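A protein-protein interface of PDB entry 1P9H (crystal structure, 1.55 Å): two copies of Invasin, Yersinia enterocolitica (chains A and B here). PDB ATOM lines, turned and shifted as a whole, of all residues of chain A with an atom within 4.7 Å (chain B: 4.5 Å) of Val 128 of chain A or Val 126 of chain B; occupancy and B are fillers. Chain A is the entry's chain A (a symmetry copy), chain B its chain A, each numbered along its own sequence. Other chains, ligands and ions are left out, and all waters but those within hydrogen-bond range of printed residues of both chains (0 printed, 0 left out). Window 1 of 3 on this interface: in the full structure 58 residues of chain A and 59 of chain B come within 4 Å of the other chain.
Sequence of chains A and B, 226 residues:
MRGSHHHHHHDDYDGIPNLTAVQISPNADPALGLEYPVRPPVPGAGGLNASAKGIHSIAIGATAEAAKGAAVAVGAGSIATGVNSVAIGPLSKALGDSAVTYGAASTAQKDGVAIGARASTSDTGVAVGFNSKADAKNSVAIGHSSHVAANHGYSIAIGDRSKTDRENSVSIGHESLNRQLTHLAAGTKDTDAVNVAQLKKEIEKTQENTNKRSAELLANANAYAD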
ATOM      1  N   ILE A 115     -22.962   3.788 -18.888  1.00  0.00           N
ATOM      2  CA  ILE A 115     -23.950   3.298 -17.927  1.00  0.00           C
ATOM      3  C   ILE A 115     -25.353   3.322 -18.526  1.00  0.00           C
ATOM      4  O   ILE A 115     -25.843   4.375 -18.934  1.00  0.00           O
ATOM      5  CB  ILE A 115     -23.950   4.179 -16.656  1.00  0.00           C
ATOM      6  CG1 ILE A 115     -22.521   4.351 -16.126  1.00  0.00           C
ATOM      7  CG2 ILE A 115     -24.846   3.561 -15.593  1.00  0.00           C
ATOM      8  CD1 ILE A 115     -21.838   3.051 -15.726  1.00  0.00           C
ATOM      9  N   VAL A 126     -17.996   9.690 -21.524  1.00  0.00           N
ATOM     10  CA  VAL A 126     -18.994   9.311 -20.532  1.00  0.00           C
ATOM     11  C   VAL A 126     -20.360   9.271 -21.197  1.00  0.00           C
ATOM     12  O   VAL A 126     -20.788  10.245 -21.816  1.00  0.00           O
ATOM     13  CB  VAL A 126     -19.063  10.325 -19.369  1.00  0.00           C
ATOM     14  CG1 VAL A 126     -20.229   9.971 -18.446  1.00  0.00           C
ATOM     15  CG2 VAL A 126     -17.755  10.329 -18.593  1.00  0.00           C
ATOM     16  N   ALA A 127     -21.032   8.132 -21.081  1.00  0.00           N
ATOM     17  CA  ALA A 127     -22.366   7.970 -21.638  1.00  0.00           C
ATOM     18  C   ALA A 127     -23.235   7.372 -20.541  1.00  0.00           C
ATOM     19  O   ALA A 127     -22.953   6.282 -20.050  1.00  0.00           O
ATOM     20  CB  ALA A 127     -22.333   7.038 -22.855  1.00  0.00           C
ATOM     21  N   VAL A 128     -24.265   8.106 -20.133  1.00  0.00           N
ATOM     22  CA  VAL A 128     -25.177   7.618 -19.107  1.00  0.00           C
ATOM     23  C   VAL A 128     -26.599   7.765 -19.621  1.00  0.00           C
ATOM     24  O   VAL A 128     -27.035   8.866 -19.961  1.00  0.00           O
ATOM     25  CB  VAL A 128     -25.048   8.406 -17.787  1.00  0.00           C
ATOM     26  CG1 VAL A 128     -25.989   7.809 -16.741  1.00  0.00           C
ATOM     27  CG2 VAL A 128     -23.617   8.352 -17.276  1.00  0.00           C
ATOM     28  N   GLY A 129     -27.317   6.649 -19.681  1.00  0.00           N
ATOM     29  CA  GLY A 129     -28.683   6.668 -20.164  1.00  0.00           C
ATOM     30  C   GLY A 129     -28.905   5.611 -21.225  1.00  0.00           C
ATOM     31  O   GLY A 129     -27.976   5.226 -21.938  1.00  0.00           O
ATOM     32  N   SER A 132     -27.586   6.062 -24.861  1.00  0.00           N
ATOM     33  CA  SER A 132     -26.801   7.294 -24.894  1.00  0.00           C
ATOM     34  C   SER A 132     -25.549   7.004 -25.719  1.00  0.00           C
ATOM     35  O   SER A 132     -25.036   5.881 -25.704  1.00  0.00           O
ATOM     36  CB  SER A 132     -26.423   7.735 -23.471  1.00  0.00           C
ATOM     37  OG  SER A 132     -25.720   6.724 -22.769  1.00  0.00           O
ATOM     38  N   ALA A 141     -22.384  12.311 -22.773  1.00  0.00           N
ATOM     39  CA  ALA A 141     -23.772  12.226 -23.203  1.00  0.00           C
ATOM     40  C   ALA A 141     -24.591  11.683 -22.041  1.00  0.00           C
ATOM     41  O   ALA A 141     -24.446  10.516 -21.672  1.00  0.00           O
ATOM     42  CB  ALA A 141     -23.891  11.303 -24.414  1.00  0.00           C
ATOM     43  N   ILE A 142     -25.439  12.531 -21.460  1.00  0.00           N
ATOM     44  CA  ILE A 142     -26.271  12.134 -20.326  1.00  0.00           C
ATOM     45  C   ILE A 142     -27.742  12.242 -20.690  1.00  0.00           C
ATOM     46  O   ILE A 142     -28.231  13.326 -21.012  1.00  0.00           O
ATOM     47  CB  ILE A 142     -26.027  13.040 -19.088  1.00  0.00           C
ATOM     48  CG1 ILE A 142     -24.529  13.142 -18.781  1.00  0.00           C
ATOM     49  CG2 ILE A 142     -26.777  12.482 -17.883  1.00  0.00           C
ATOM     50  CD1 ILE A 142     -23.872  11.830 -18.395  1.00  0.00           C
ATOM     51  N   GLY A 143     -28.450  11.116 -20.627  1.00  0.00           N
ATOM     52  CA  GLY A 143     -29.861  11.106 -20.949  1.00  0.00           C
ATOM     53  C   GLY A 143     -30.197  10.094 -22.023  1.00  0.00           C
ATOM     54  O   GLY A 143     -29.337   9.716 -22.826  1.00  0.00           O
ATOM     55  N   HIS A 144     -31.446   9.641 -22.034  1.00  0.00           N
ATOM     56  CA  HIS A 144     -31.896   8.680 -23.035  1.00  0.00           C
ATOM     57  C   HIS A 144     -31.639   9.201 -24.446  1.00  0.00           C
ATOM     58  O   HIS A 144     -32.066  10.296 -24.805  1.00  0.00           O
ATOM     59  CB  HIS A 144     -33.392   8.401 -22.877  1.00  0.00           C
ATOM     60  CG  HIS A 144     -34.011   7.772 -24.086  1.00  0.00           C
ATOM     61  ND1 HIS A 144     -34.952   8.416 -24.861  1.00  0.00           N
ATOM     62  CD2 HIS A 144     -33.808   6.566 -24.668  1.00  0.00           C
ATOM     63  CE1 HIS A 144     -35.301   7.636 -25.868  1.00  0.00           C
ATOM     64  NE2 HIS A 144     -34.621   6.507 -25.774  1.00  0.00           N
ATOM     65  N   SER A 146     -29.179  10.507 -25.790  1.00  0.00           N
ATOM     66  CA  SER A 146     -28.416  11.746 -25.895  1.00  0.00           C
ATOM     67  C   SER A 146     -27.293  11.387 -26.859  1.00  0.00           C
ATOM     68  O   SER A 146     -26.875  10.227 -26.926  1.00  0.00           O
ATOM     69  CB  SER A 146     -27.864  12.170 -24.527  1.00  0.00           C
ATOM     70  OG  SER A 146     -27.156  11.124 -23.885  1.00  0.00           O
ATOM     71  N   VAL B 113     -32.033   4.322 -15.674  1.00  0.00           N
ATOM     72  CA  VAL B 113     -30.725   4.225 -15.031  1.00  0.00           C
ATOM     73  C   VAL B 113     -30.813   4.920 -13.672  1.00  0.00           C
ATOM     74  O   VAL B 113     -31.172   6.095 -13.597  1.00  0.00           O
ATOM     75  CB  VAL B 113     -29.623   4.933 -15.864  1.00  0.00           C
ATOM     76  CG1 VAL B 113     -28.315   4.986 -15.073  1.00  0.00           C
ATOM     77  CG2 VAL B 113     -29.416   4.212 -17.187  1.00  0.00           C
ATOM     78  N   THR B 121     -35.646   6.342 -10.620  1.00  0.00           N
ATOM     79  CA  THR B 121     -35.987   6.892 -11.919  1.00  0.00           C
ATOM     80  C   THR B 121     -37.200   6.236 -12.543  1.00  0.00           C
ATOM     81  O   THR B 121     -37.460   5.041 -12.347  1.00  0.00           O
ATOM     82  CB  THR B 121     -34.825   6.765 -12.932  1.00  0.00           C
ATOM     83  OG1 THR B 121     -35.224   7.346 -14.183  1.00  0.00           O
ATOM     84  CG2 THR B 121     -34.471   5.305 -13.172  1.00  0.00           C
ATOM     85  N   GLY B 125     -35.527   7.122 -17.798  1.00  0.00           N
ATOM     86  CA  GLY B 125     -34.896   8.274 -17.183  1.00  0.00           C
ATOM     87  C   GLY B 125     -33.507   7.965 -16.665  1.00  0.00           C
ATOM     88  O   GLY B 125     -33.013   6.842 -16.796  1.00  0.00           O
ATOM     89  N   VAL B 126     -32.871   8.976 -16.085  1.00  0.00           N
ATOM     90  CA  VAL B 126     -31.537   8.829 -15.518  1.00  0.00           C
ATOM     91  C   VAL B 126     -31.484   9.558 -14.187  1.00  0.00           C
ATOM     92  O   VAL B 126     -31.805  10.743 -14.105  1.00  0.00           O
ATOM     93  CB  VAL B 126     -30.452   9.435 -16.435  1.00  0.00           C
ATOM     94  CG1 VAL B 126     -29.099   9.400 -15.724  1.00  0.00           C
ATOM     95  CG2 VAL B 126     -30.381   8.672 -17.748  1.00  0.00           C
ATOM     96  N   ALA B 127     -31.095   8.837 -13.141  1.00  0.00           N
ATOM     97  CA  ALA B 127     -30.965   9.419 -11.815  1.00  0.00           C
ATOM     98  C   ALA B 127     -29.605   9.000 -11.278  1.00  0.00           C
ATOM     99  O   ALA B 127     -29.331   7.810 -11.139  1.00  0.00           O
ATOM    100  CB  ALA B 127     -32.078   8.912 -10.891  1.00  0.00           C
ATOM    101  N   VAL B 128     -28.742   9.976 -11.017  1.00  0.00           N
ATOM    102  CA  VAL B 128     -27.421   9.688 -10.475  1.00  0.00           C
ATOM    103  C   VAL B 128     -27.203  10.565  -9.253  1.00  0.00           C
ATOM    104  O   VAL B 128     -27.271  11.792  -9.339  1.00  0.00           O
ATOM    105  CB  VAL B 128     -26.295   9.974 -11.491  1.00  0.00           C
ATOM    106  CG1 VAL B 128     -24.947   9.599 -10.879  1.00  0.00           C
ATOM    107  CG2 VAL B 128     -26.518   9.175 -12.764  1.00  0.00           C
ATOM    108  N   ALA B 134     -35.677  11.057 -10.701  1.00  0.00           N
ATOM    109  CA  ALA B 134     -36.073  11.420 -12.058  1.00  0.00           C
ATOM    110  C   ALA B 134     -37.497  10.891 -12.180  1.00  0.00           C
ATOM    111  O   ALA B 134     -37.740   9.852 -12.798  1.00  0.00           O
ATOM    112  CB  ALA B 134     -35.159  10.739 -13.069  1.00  0.00           C
ATOM    113  N   SER B 139     -36.773  11.852 -17.850  1.00  0.00           N
ATOM    114  CA  SER B 139     -36.079  12.950 -17.183  1.00  0.00           C
ATOM    115  C   SER B 139     -34.682  12.554 -16.712  1.00  0.00           C
ATOM    116  O   SER B 139     -34.323  11.373 -16.708  1.00  0.00           O
ATOM    117  CB  SER B 139     -36.905  13.475 -16.000  1.00  0.00           C
ATOM    118  OG  SER B 139     -37.086  12.485 -15.001  1.00  0.00           O
ATOM    119  N   VAL B 140     -33.897  13.557 -16.330  1.00  0.00           N
ATOM    120  CA  VAL B 140     -32.526  13.358 -15.866  1.00  0.00           C
ATOM    121  C   VAL B 140     -32.304  14.150 -14.585  1.00  0.00           C
ATOM    122  O   VAL B 140     -32.543  15.354 -14.547  1.00  0.00           O
ATOM    123  CB  VAL B 140     -31.505  13.848 -16.925  1.00  0.00           C
ATOM    124  CG1 VAL B 140     -30.083  13.750 -16.379  1.00  0.00           C
ATOM    125  CG2 VAL B 140     -31.641  13.027 -18.200  1.00  0.00           C
ATOM    126  N   ALA B 141     -31.846  13.466 -13.541  1.00  0.00           N
ATOM    127  CA  ALA B 141     -31.577  14.106 -12.262  1.00  0.00           C
ATOM    128  C   ALA B 141     -30.181  13.695 -11.817  1.00  0.00           C
ATOM    129  O   ALA B 141     -29.954  12.530 -11.486  1.00  0.00           O
ATOM    130  CB  ALA B 141     -32.613  13.671 -11.228  1.00  0.00           C
ATOM    131  N   ILE B 142     -29.249  14.646 -11.821  1.00  0.00           N
ATOM    132  CA  ILE B 142     -27.867  14.376 -11.428  1.00  0.00           C
ATOM    133  C   ILE B 142     -27.495  15.201 -10.208  1.00  0.00           C
ATOM    134  O   ILE B 142     -27.522  16.431 -10.252  1.00  0.00           O
ATOM    135  CB  ILE B 142     -26.865  14.734 -12.560  1.00  0.00           C
ATOM    136  CG1 ILE B 142     -27.294  14.093 -13.884  1.00  0.00           C
ATOM    137  CG2 ILE B 142     -25.465  14.269 -12.177  1.00  0.00           C
ATOM    138  CD1 ILE B 142     -27.296  12.575 -13.880  1.00  0.00           C
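The side-chain hydroxyl (OG) of Ser 132 of chain A sits at hydrogen-bond distance from the backbone carbonyl oxygen (O) of Gly 129 of chain A (2.8 Å).
The backbone NH (N) of Ile 142 of chain A sits at hydrogen-bond distance from the side-chain hydroxyl (OG) of Ser 146 of chain A (3.3 Å).
The backbone carbonyl oxygen (O) of Gly 143 of chain A is in hydrogen-bond range of the side-chain hydroxyl (OG) of Ser 146 of chain A (2.8 Å).
The backbone carbonyl oxygen of Gly 125 of chain B lies within hydrogen-bond range of the backbone NH of Val 113 of chain B, at 2.9 Å.
The backbone carbonyl oxygen (O) of Ile 115 of chain A lies within hydrogen-bond range of the backbone NH (N) of Gly 129 of chain A (2.8 Å).
N of Ala 127 of chain B sits at hydrogen-bond distance from O of Val 113 of chain B, 2.8 Å away.
Val 113 of chain B touches Ile 115 of chain A (CG1 to CG2, 3.8 Å).
Val 128 of chain A touches Val 126 of chain B (CG1 to CG1, 3.6 Å).
CA of Gly 129 of chain A touches CG2 of Val 113 of chain B, 3.9 Å away.
Gly 129 of chain A touches Val 126 of chain B.
Val 140 of chain B touches Ile 142 of chain A.
Gly 143 of chain A touches Val 140 of chain B (CA to CG2, 3.8 Å).
Val 128 of chain A touches just one residue of chain B: Val 126 (3.6 Å).
Of chain A, only Val 128 and Gly 129 come within 4 Å of Val 126 of chain B.
Of the printed residues of chain B, Ile 115 of chain A touches Val 113 (3.8 Å).
Printed residues of chain B within 4 Å of Ile 142 of chain A: Val 140 (3.8 Å).
Of the printed residues of chain A, Val 140 of chain B touches Ile 142 and Gly 143.
Printed residues of chain B within 4 Å of Gly 129 of chain A: Val 113 (3.9 Å) and Val 126 (3.6 Å).
His 144 of chain A touches none of the printed residues of chain B.
Val 126 of chain A touches none of the printed residues of chain B.
The nearest residue of chain A that does not touch Val 126 of chain B is Gly 143 of chain A (4.1 Å).
The nearest printed residue of chain B that does not touch Ile 142 of chain A is Ile 142 of chain B (4.04 Å).
Of the 11 printed residues of chain B, 3 touch a printed residue of chain A.
Printed residues of chain B that touch a printed residue of chain A: Val 113, Val 126 and Val 140.
Along chain B the printed residues that touch a printed residue of chain A span positions 113 to 140.
Of the 11 printed residues of chain A, 5 touch a printed residue of chain B.
Hydrophobic or aromatic side chains of chain A that line the printed part of chain B: Ile 115, Val 128 and Ile 142.
Val 128 of chain A touches Val 126 of chain B, but with the chains exchanged Val 126 of chain A does not touch Val 128 of chain B (8.5 Å).
Of the 6 pairs that touch across the chains among the printed residues, none has its exchanged pair printed and touching as well.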
